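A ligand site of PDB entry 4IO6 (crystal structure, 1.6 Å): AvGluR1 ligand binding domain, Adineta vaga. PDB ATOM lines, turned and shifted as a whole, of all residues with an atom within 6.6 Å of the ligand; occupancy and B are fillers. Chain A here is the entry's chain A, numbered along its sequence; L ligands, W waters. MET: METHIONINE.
Residues that only touch the ligand: Thr 139 (3.4 Å), Met 107 (3.4 Å), Tyr 67 (3.4 Å), Ile 86 (3.7 Å), Arg 136 (3.7 Å), Met 179 (3.8 Å) and Phe 207 (3.8 Å). Hydrophobic or aromatic side chains within 4 Å of the ligand: Tyr 67, Met 107, Ala 140 and Phe 207. 13 residues have an atom within 4 Å of the ligand: Tyr 67, Asp 85, Ile 86, Thr 87, Arg 92, Met 107, Arg 136, Thr 139, Ala 140, Gly 141, Met 179, Asp 180 and Phe 207. Along chain A the residues within 4 Å of the ligand span positions 67 to 207.
ND2 of Asn 105 is in hydrogen-bond range of OD1 of Asp 180 (3.0 Å). The backbone carbonyl oxygen (O) of Asp 180 is in hydrogen-bond range of the side-chain hydroxyl (OG1) of Thr 183. The guanidinium group of Arg 92 sits at hydrogen-bond distance from the backbone carbonyl oxygen of Thr 87. The backbone NH of Arg 92 lies within hydrogen-bond range of the side-chain hydroxyl of Thr 89. OH of Tyr 67 sits at hydrogen-bond distance from OD1 of Asp 85 (2.7 Å). The backbone carbonyl oxygen of Arg 136 sits at hydrogen-bond distance from the side-chain hydroxyl of Thr 139, at 2.7 Å. The backbone NH (N) of Glu 142 is in hydrogen-bond range of the side-chain hydroxyl (OG1) of Thr 139, 3.3 Å away. NH2 of Arg 162 is in hydrogen-bond range of OH of Tyr 67 (3.0 Å).
Water W1 bridges the side-chain hydroxyl of Thr 139 (2.9 Å) and a sulfur (SD) of the ligand (3.3 Å).
The side-chain carboxylate (OD2) of Asp 180 is in salt-bridge range of a nitrogen (N) of the ligand. The backbone NH (N) of Thr 87 sits at hydrogen-bond distance from an oxygen (O) of the ligand (2.9 Å). A nitrogen (N) of the ligand lies within hydrogen-bond range of the side-chain hydroxyl (OG1) of Thr 87, at 2.8 Å. The guanidinium group of Arg 92 lies within salt-bridge range of an oxygen (O) of the ligand, 2.8 Å away. OXT of the ligand is in hydrogen-bond range of N of Ala 140 (2.8 Å). The backbone carbonyl oxygen (O) of Asp 85 is in hydrogen-bond range of a nitrogen (N) of the ligand (2.8 Å). A sulfur (SD) of the ligand sits close to the backbone NH of Gly 141 (3.6 Å).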
ATOM      1  N   TYR A  67     -21.570 -29.817 -23.583  1.00  0.00           N
ATOM      2  CA  TYR A  67     -21.189 -28.418 -23.719  1.00  0.00           C
ATOM      3  C   TYR A  67     -21.281 -28.005 -25.182  1.00  0.00           C
ATOM      4  O   TYR A  67     -21.789 -26.913 -25.513  1.00  0.00           O
ATOM      5  CB  TYR A  67     -19.805 -28.154 -23.104  1.00  0.00           C
ATOM      6  CG  TYR A  67     -19.916 -28.110 -21.606  1.00  0.00           C
ATOM      7  CD1 TYR A  67     -19.999 -29.250 -20.854  1.00  0.00           C
ATOM      8  CD2 TYR A  67     -20.016 -26.894 -20.938  1.00  0.00           C
ATOM      9  CE1 TYR A  67     -20.156 -29.200 -19.468  1.00  0.00           C
ATOM     10  CE2 TYR A  67     -20.172 -26.822 -19.572  1.00  0.00           C
ATOM     11  CZ  TYR A  67     -20.253 -27.989 -18.833  1.00  0.00           C
ATOM     12  OH  TYR A  67     -20.425 -27.924 -17.456  1.00  0.00           O
ATOM     13  N   THR A  68     -20.835 -28.863 -26.098  1.00  0.00           N
ATOM     14  CA  THR A  68     -20.991 -28.549 -27.527  1.00  0.00           C
ATOM     15  C   THR A  68     -22.469 -28.430 -27.866  1.00  0.00           C
ATOM     16  O   THR A  68     -22.877 -27.583 -28.666  1.00  0.00           O
ATOM     17  CB  THR A  68     -20.388 -29.665 -28.369  1.00  0.00           C
ATOM     18  OG1 THR A  68     -18.974 -29.584 -28.245  1.00  0.00           O
ATOM     19  CG2 THR A  68     -20.838 -29.541 -29.843  1.00  0.00           C
ATOM     20  N   ASP A  85     -19.685 -22.824 -17.128  1.00  0.00           N
ATOM     21  CA  ASP A  85     -18.288 -23.194 -17.202  1.00  0.00           C
ATOM     22  C   ASP A  85     -18.007 -23.674 -18.625  1.00  0.00           C
ATOM     23  O   ASP A  85     -17.698 -24.840 -18.882  1.00  0.00           O
ATOM     24  CB  ASP A  85     -17.957 -24.228 -16.122  1.00  0.00           C
ATOM     25  CG  ASP A  85     -18.902 -25.439 -16.094  1.00  0.00           C
ATOM     26  OD1 ASP A  85     -20.043 -25.412 -16.603  1.00  0.00           O
ATOM     27  OD2 ASP A  85     -18.505 -26.466 -15.431  1.00  0.00           O
ATOM     28  N   ILE A  86     -18.157 -22.732 -19.556  1.00  0.00           N
ATOM     29  CA  ILE A  86     -18.147 -22.980 -20.972  1.00  0.00           C
ATOM     30  C   ILE A  86     -16.843 -22.453 -21.577  1.00  0.00           C
ATOM     31  O   ILE A  86     -16.574 -21.270 -21.583  1.00  0.00           O
ATOM     32  CB  ILE A  86     -19.353 -22.304 -21.680  1.00  0.00           C
ATOM     33  CG1 ILE A  86     -20.685 -22.706 -21.040  1.00  0.00           C
ATOM     34  CG2 ILE A  86     -19.321 -22.650 -23.143  1.00  0.00           C
ATOM     35  CD1 ILE A  86     -21.876 -21.852 -21.517  1.00  0.00           C
ATOM     36  N   THR A  87     -15.997 -23.364 -22.046  1.00  0.00           N
ATOM     37  CA  THR A  87     -14.704 -23.023 -22.546  1.00  0.00           C
ATOM     38  C   THR A  87     -14.775 -22.368 -23.927  1.00  0.00           C
ATOM     39  O   THR A  87     -15.505 -22.828 -24.794  1.00  0.00           O
ATOM     40  CB  THR A  87     -13.819 -24.302 -22.617  1.00  0.00           C
ATOM     41  OG1 THR A  87     -13.780 -24.848 -21.303  1.00  0.00           O
ATOM     42  CG2 THR A  87     -12.439 -23.986 -23.051  1.00  0.00           C
ATOM     43  N   VAL A  88     -14.028 -21.280 -24.078  1.00  0.00           N
ATOM     44  CA  VAL A  88     -13.897 -20.596 -25.351  1.00  0.00           C
ATOM     45  C   VAL A  88     -12.940 -21.415 -26.201  1.00  0.00           C
ATOM     46  O   VAL A  88     -11.763 -21.618 -25.871  1.00  0.00           O
ATOM     47  CB  VAL A  88     -13.371 -19.185 -25.146  1.00  0.00           C
ATOM     48  CG1 VAL A  88     -13.257 -18.456 -26.469  1.00  0.00           C
ATOM     49  CG2 VAL A  88     -14.281 -18.403 -24.168  1.00  0.00           C
ATOM     50  N   THR A  89     -13.424 -21.887 -27.346  1.00  0.00           N
ATOM     51  CA  THR A  89     -12.583 -22.617 -28.280  1.00  0.00           C
ATOM     52  C   THR A  89     -12.712 -22.064 -29.693  1.00  0.00           C
ATOM     53  O   THR A  89     -13.716 -21.453 -30.030  1.00  0.00           O
ATOM     54  CB  THR A  89     -12.949 -24.134 -28.335  1.00  0.00           C
ATOM     55  OG1 THR A  89     -14.185 -24.304 -29.050  1.00  0.00           O
ATOM     56  CG2 THR A  89     -13.112 -24.703 -26.913  1.00  0.00           C
ATOM     57  N   ARG A  92     -15.797 -23.415 -31.596  1.00  0.00           N
ATOM     58  CA  ARG A  92     -17.040 -22.802 -31.193  1.00  0.00           C
ATOM     59  C   ARG A  92     -17.148 -21.373 -31.675  1.00  0.00           C
ATOM     60  O   ARG A  92     -18.232 -20.912 -32.014  1.00  0.00           O
ATOM     61  CB  ARG A  92     -17.158 -22.834 -29.677  1.00  0.00           C
ATOM     62  CG  ARG A  92     -17.333 -24.255 -29.141  1.00  0.00           C
ATOM     63  CD  ARG A  92     -17.127 -24.345 -27.638  1.00  0.00           C
ATOM     64  NE  ARG A  92     -17.268 -25.737 -27.179  1.00  0.00           N
ATOM     65  CZ  ARG A  92     -17.216 -26.141 -25.905  1.00  0.00           C
ATOM     66  NH1 ARG A  92     -17.006 -25.268 -24.938  1.00  0.00           N
ATOM     67  NH2 ARG A  92     -17.345 -27.434 -25.602  1.00  0.00           N
ATOM     68  N   ASN A 105      -9.084 -20.667 -16.875  1.00  0.00           N
ATOM     69  CA  ASN A 105      -9.387 -22.091 -16.721  1.00  0.00           C
ATOM     70  C   ASN A 105      -8.175 -22.872 -17.194  1.00  0.00           C
ATOM     71  O   ASN A 105      -7.304 -22.350 -17.881  1.00  0.00           O
ATOM     72  CB  ASN A 105     -10.597 -22.485 -17.568  1.00  0.00           C
ATOM     73  CG  ASN A 105     -11.012 -23.913 -17.354  1.00  0.00           C
ATOM     74  OD1 ASN A 105     -11.153 -24.354 -16.215  1.00  0.00           O
ATOM     75  ND2 ASN A 105     -11.158 -24.665 -18.445  1.00  0.00           N
ATOM     76  N   SER A 106      -8.127 -24.119 -16.752  1.00  0.00           N
ATOM     77  CA  SER A 106      -7.174 -25.126 -17.261  1.00  0.00           C
ATOM     78  C   SER A 106      -7.807 -26.463 -16.877  1.00  0.00           C
ATOM     79  O   SER A 106      -8.804 -26.505 -16.144  1.00  0.00           O
ATOM     80  CB  SER A 106      -5.781 -24.940 -16.644  1.00  0.00           C
ATOM     81  OG  SER A 106      -5.840 -24.965 -15.224  1.00  0.00           O
ATOM     82  N   MET A 107      -7.246 -27.574 -17.348  1.00  0.00           N
ATOM     83  CA  MET A 107      -7.752 -28.906 -17.023  1.00  0.00           C
ATOM     84  C   MET A 107      -6.809 -29.674 -16.119  1.00  0.00           C
ATOM     85  O   MET A 107      -5.591 -29.405 -16.091  1.00  0.00           O
ATOM     86  CB  MET A 107      -8.030 -29.693 -18.291  1.00  0.00           C
ATOM     87  CG  MET A 107      -9.234 -29.177 -19.038  1.00  0.00           C
ATOM     88  SD  MET A 107      -9.736 -30.287 -20.388  1.00  0.00           S
ATOM     89  CE  MET A 107      -8.721 -29.728 -21.725  1.00  0.00           C
ATOM     90  N   ARG A 108      -7.364 -30.637 -15.395  1.00  0.00           N
ATOM     91  CA  ARG A 108      -6.602 -31.563 -14.560  1.00  0.00           C
ATOM     92  C   ARG A 108      -6.996 -32.996 -14.883  1.00  0.00           C
ATOM     93  O   ARG A 108      -8.118 -33.250 -15.339  1.00  0.00           O
ATOM     94  CB  ARG A 108      -6.896 -31.353 -13.065  1.00  0.00           C
ATOM     95  CG  ARG A 108      -6.582 -29.968 -12.471  1.00  0.00           C
ATOM     96  CD  ARG A 108      -5.118 -29.632 -12.360  1.00  0.00           C
ATOM     97  NE  ARG A 108      -4.220 -30.656 -11.807  1.00  0.00           N
ATOM     98  CZ  ARG A 108      -3.942 -30.850 -10.515  1.00  0.00           C
ATOM     99  NH1 ARG A 108      -4.536 -30.133  -9.561  1.00  0.00           N
ATOM    100  NH2 ARG A 108      -3.071 -31.801 -10.165  1.00  0.00           N
ATOM    101  N   ARG A 136     -15.649 -37.288 -21.746  1.00  0.00           N
ATOM    102  CA  ARG A 136     -17.009 -36.799 -21.957  1.00  0.00           C
ATOM    103  C   ARG A 136     -17.135 -36.242 -23.399  1.00  0.00           C
ATOM    104  O   ARG A 136     -16.418 -35.333 -23.782  1.00  0.00           O
ATOM    105  CB  ARG A 136     -17.371 -35.716 -20.940  1.00  0.00           C
ATOM    106  CG  ARG A 136     -17.719 -36.287 -19.588  1.00  0.00           C
ATOM    107  CD  ARG A 136     -17.890 -35.135 -18.593  1.00  0.00           C
ATOM    108  NE  ARG A 136     -16.581 -34.654 -18.161  1.00  0.00           N
ATOM    109  CZ  ARG A 136     -16.322 -33.423 -17.695  1.00  0.00           C
ATOM    110  NH1 ARG A 136     -17.257 -32.486 -17.661  1.00  0.00           N
ATOM    111  NH2 ARG A 136     -15.094 -33.137 -17.310  1.00  0.00           N
ATOM    112  N   GLY A 138     -18.342 -34.161 -26.591  1.00  0.00           N
ATOM    113  CA  GLY A 138     -18.869 -32.819 -26.730  1.00  0.00           C
ATOM    114  C   GLY A 138     -18.342 -31.885 -25.678  1.00  0.00           C
ATOM    115  O   GLY A 138     -19.053 -31.015 -25.195  1.00  0.00           O
ATOM    116  N   THR A 139     -17.078 -32.075 -25.296  1.00  0.00           N
ATOM    117  CA  THR A 139     -16.404 -31.187 -24.357  1.00  0.00           C
ATOM    118  C   THR A 139     -15.026 -30.812 -24.866  1.00  0.00           C
ATOM    119  O   THR A 139     -14.442 -31.483 -25.734  1.00  0.00           O
ATOM    120  CB  THR A 139     -16.200 -31.816 -22.961  1.00  0.00           C
ATOM    121  OG1 THR A 139     -15.288 -32.928 -23.074  1.00  0.00           O
ATOM    122  CG2 THR A 139     -17.532 -32.249 -22.391  1.00  0.00           C
ATOM    123  N   ALA A 140     -14.454 -29.781 -24.260  1.00  0.00           N
ATOM    124  CA  ALA A 140     -13.067 -29.437 -24.545  1.00  0.00           C
ATOM    125  C   ALA A 140     -12.062 -30.552 -24.202  1.00  0.00           C
ATOM    126  O   ALA A 140     -10.956 -30.602 -24.774  1.00  0.00           O
ATOM    127  CB  ALA A 140     -12.693 -28.112 -23.818  1.00  0.00           C
ATOM    128  N   GLY A 141     -12.424 -31.438 -23.283  1.00  0.00           N
ATOM    129  CA  GLY A 141     -11.581 -32.576 -22.941  1.00  0.00           C
ATOM    130  C   GLY A 141     -11.477 -33.526 -24.134  1.00  0.00           C
ATOM    131  O   GLY A 141     -10.404 -34.079 -24.411  1.00  0.00           O
ATOM    132  N   GLU A 142     -12.586 -33.708 -24.830  1.00  0.00           N
ATOM    133  CA  GLU A 142     -12.569 -34.516 -26.055  1.00  0.00           C
ATOM    134  C   GLU A 142     -11.661 -33.858 -27.107  1.00  0.00           C
ATOM    135  O   GLU A 142     -10.877 -34.527 -27.763  1.00  0.00           O
ATOM    136  CB  GLU A 142     -13.961 -34.736 -26.601  1.00  0.00           C
ATOM    137  CG  GLU A 142     -13.967 -35.638 -27.842  1.00  0.00           C
ATOM    138  CD  GLU A 142     -15.313 -35.800 -28.523  1.00  0.00           C
ATOM    139  OE1 GLU A 142     -16.211 -34.923 -28.405  1.00  0.00           O
ATOM    140  OE2 GLU A 142     -15.418 -36.784 -29.290  1.00  0.00           O
ATOM    141  N   ASP A 143     -11.808 -32.551 -27.274  1.00  0.00           N
ATOM    142  CA  ASP A 143     -11.002 -31.837 -28.251  1.00  0.00           C
ATOM    143  C   ASP A 143      -9.507 -32.021 -27.982  1.00  0.00           C
ATOM    144  O   ASP A 143      -8.718 -32.298 -28.895  1.00  0.00           O
ATOM    145  CB  ASP A 143     -11.316 -30.357 -28.204  1.00  0.00           C
ATOM    146  CG  ASP A 143     -12.757 -30.017 -28.557  1.00  0.00           C
ATOM    147  OD1 ASP A 143     -13.143 -28.890 -28.231  1.00  0.00           O
ATOM    148  OD2 ASP A 143     -13.486 -30.839 -29.159  1.00  0.00           O
ATOM    149  N   ARG A 162     -20.882 -35.907 -16.232  1.00  0.00           N
ATOM    150  CA  ARG A 162     -19.951 -36.020 -15.119  1.00  0.00           C
ATOM    151  C   ARG A 162     -20.344 -37.193 -14.233  1.00  0.00           C
ATOM    152  O   ARG A 162     -19.490 -37.872 -13.711  1.00  0.00           O
ATOM    153  CB  ARG A 162     -19.889 -34.740 -14.303  1.00  0.00           C
ATOM    154  CG  ARG A 162     -19.155 -33.639 -15.009  1.00  0.00           C
ATOM    155  CD  ARG A 162     -18.976 -32.425 -14.131  1.00  0.00           C
ATOM    156  NE  ARG A 162     -18.330 -31.322 -14.811  1.00  0.00           N
ATOM    157  CZ  ARG A 162     -18.937 -30.406 -15.552  1.00  0.00           C
ATOM    158  NH1 ARG A 162     -20.259 -30.450 -15.762  1.00  0.00           N
ATOM    159  NH2 ARG A 162     -18.200 -29.476 -16.160  1.00  0.00           N
ATOM    160  N   PHE A 178     -10.648 -36.306 -17.453  1.00  0.00           N
ATOM    161  CA  PHE A 178     -10.214 -34.908 -17.396  1.00  0.00           C
ATOM    162  C   PHE A 178     -11.336 -34.061 -16.837  1.00  0.00           C
ATOM    163  O   PHE A 178     -12.523 -34.304 -17.142  1.00  0.00           O
ATOM    164  CB  PHE A 178      -9.906 -34.334 -18.780  1.00  0.00           C
ATOM    165  CG  PHE A 178      -8.838 -35.068 -19.557  1.00  0.00           C
ATOM    166  CD1 PHE A 178      -7.815 -35.749 -18.936  1.00  0.00           C
ATOM    167  CD2 PHE A 178      -8.852 -35.000 -20.962  1.00  0.00           C
ATOM    168  CE1 PHE A 178      -6.836 -36.398 -19.693  1.00  0.00           C
ATOM    169  CE2 PHE A 178      -7.874 -35.626 -21.723  1.00  0.00           C
ATOM    170  CZ  PHE A 178      -6.873 -36.310 -21.098  1.00  0.00           C
ATOM    171  N   MET A 179     -10.973 -33.048 -16.043  1.00  0.00           N
ATOM    172  CA  MET A 179     -11.921 -32.056 -15.573  1.00  0.00           C
ATOM    173  C   MET A 179     -11.290 -30.668 -15.648  1.00  0.00           C
ATOM    174  O   MET A 179     -10.081 -30.518 -15.561  1.00  0.00           O
ATOM    175  CB  MET A 179     -12.305 -32.286 -14.104  1.00  0.00           C
ATOM    176  CG  MET A 179     -13.248 -33.460 -13.877  1.00  0.00           C
ATOM    177  SD  MET A 179     -13.884 -33.550 -12.185  1.00  0.00           S
ATOM    178  CE  MET A 179     -15.066 -32.192 -12.161  1.00  0.00           C
ATOM    179  N   ASP A 180     -12.139 -29.636 -15.727  1.00  0.00           N
ATOM    180  CA  ASP A 180     -11.700 -28.255 -15.496  1.00  0.00           C
ATOM    181  C   ASP A 180     -11.249 -28.104 -14.038  1.00  0.00           C
ATOM    182  O   ASP A 180     -11.773 -28.757 -13.143  1.00  0.00           O
ATOM    183  CB  ASP A 180     -12.836 -27.263 -15.767  1.00  0.00           C
ATOM    184  CG  ASP A 180     -13.279 -27.205 -17.218  1.00  0.00           C
ATOM    185  OD1 ASP A 180     -12.430 -27.362 -18.138  1.00  0.00           O
ATOM    186  OD2 ASP A 180     -14.493 -27.019 -17.449  1.00  0.00           O
ATOM    187  N   THR A 183     -13.985 -26.983 -10.948  1.00  0.00           N
ATOM    188  CA  THR A 183     -14.883 -28.073 -10.542  1.00  0.00           C
ATOM    189  C   THR A 183     -14.112 -29.305 -10.085  1.00  0.00           C
ATOM    190  O   THR A 183     -14.555 -30.019  -9.190  1.00  0.00           O
ATOM    191  CB  THR A 183     -15.879 -28.442 -11.636  1.00  0.00           C
ATOM    192  OG1 THR A 183     -15.175 -28.681 -12.869  1.00  0.00           O
ATOM    193  CG2 THR A 183     -16.883 -27.289 -11.850  1.00  0.00           C
ATOM    194  N   PHE A 207     -13.252 -19.203 -19.720  1.00  0.00           N
ATOM    195  CA  PHE A 207     -14.703 -19.379 -19.792  1.00  0.00           C
ATOM    196  C   PHE A 207     -15.307 -18.044 -20.249  1.00  0.00           C
ATOM    197  O   PHE A 207     -14.872 -16.992 -19.777  1.00  0.00           O
ATOM    198  CB  PHE A 207     -15.384 -19.725 -18.451  1.00  0.00           C
ATOM    199  CG  PHE A 207     -15.001 -21.042 -17.836  1.00  0.00           C
ATOM    200  CD1 PHE A 207     -14.640 -22.107 -18.616  1.00  0.00           C
ATOM    201  CD2 PHE A 207     -15.035 -21.226 -16.476  1.00  0.00           C
ATOM    202  CE1 PHE A 207     -14.291 -23.321 -18.056  1.00  0.00           C
ATOM    203  CE2 PHE A 207     -14.681 -22.425 -15.901  1.00  0.00           C
ATOM    204  CZ  PHE A 207     -14.334 -23.466 -16.686  1.00  0.00           C
HETATM  205  N   MET L   1     -15.572 -26.439 -19.892  1.00  0.00           N
HETATM  206  CA  MET L   1     -15.610 -27.618 -20.774  1.00  0.00           C
HETATM  207  C   MET L   1     -16.296 -27.295 -22.074  1.00  0.00           C
HETATM  208  O   MET L   1     -16.826 -26.161 -22.268  1.00  0.00           O
HETATM  209  CB  MET L   1     -16.293 -28.834 -20.121  1.00  0.00           C
HETATM  210  CG  MET L   1     -15.349 -29.595 -19.230  1.00  0.00           C
HETATM  211  SD  MET L   1     -14.095 -30.431 -20.295  1.00  0.00           S
HETATM  212  CE  MET L   1     -12.817 -30.790 -19.079  1.00  0.00           C
HETATM  213  OXT MET L   1     -16.385 -28.132 -22.981  1.00  0.00           O
HETATM  214  O   HOH W   1     -13.815 -33.745 -20.654  1.00  0.00           O
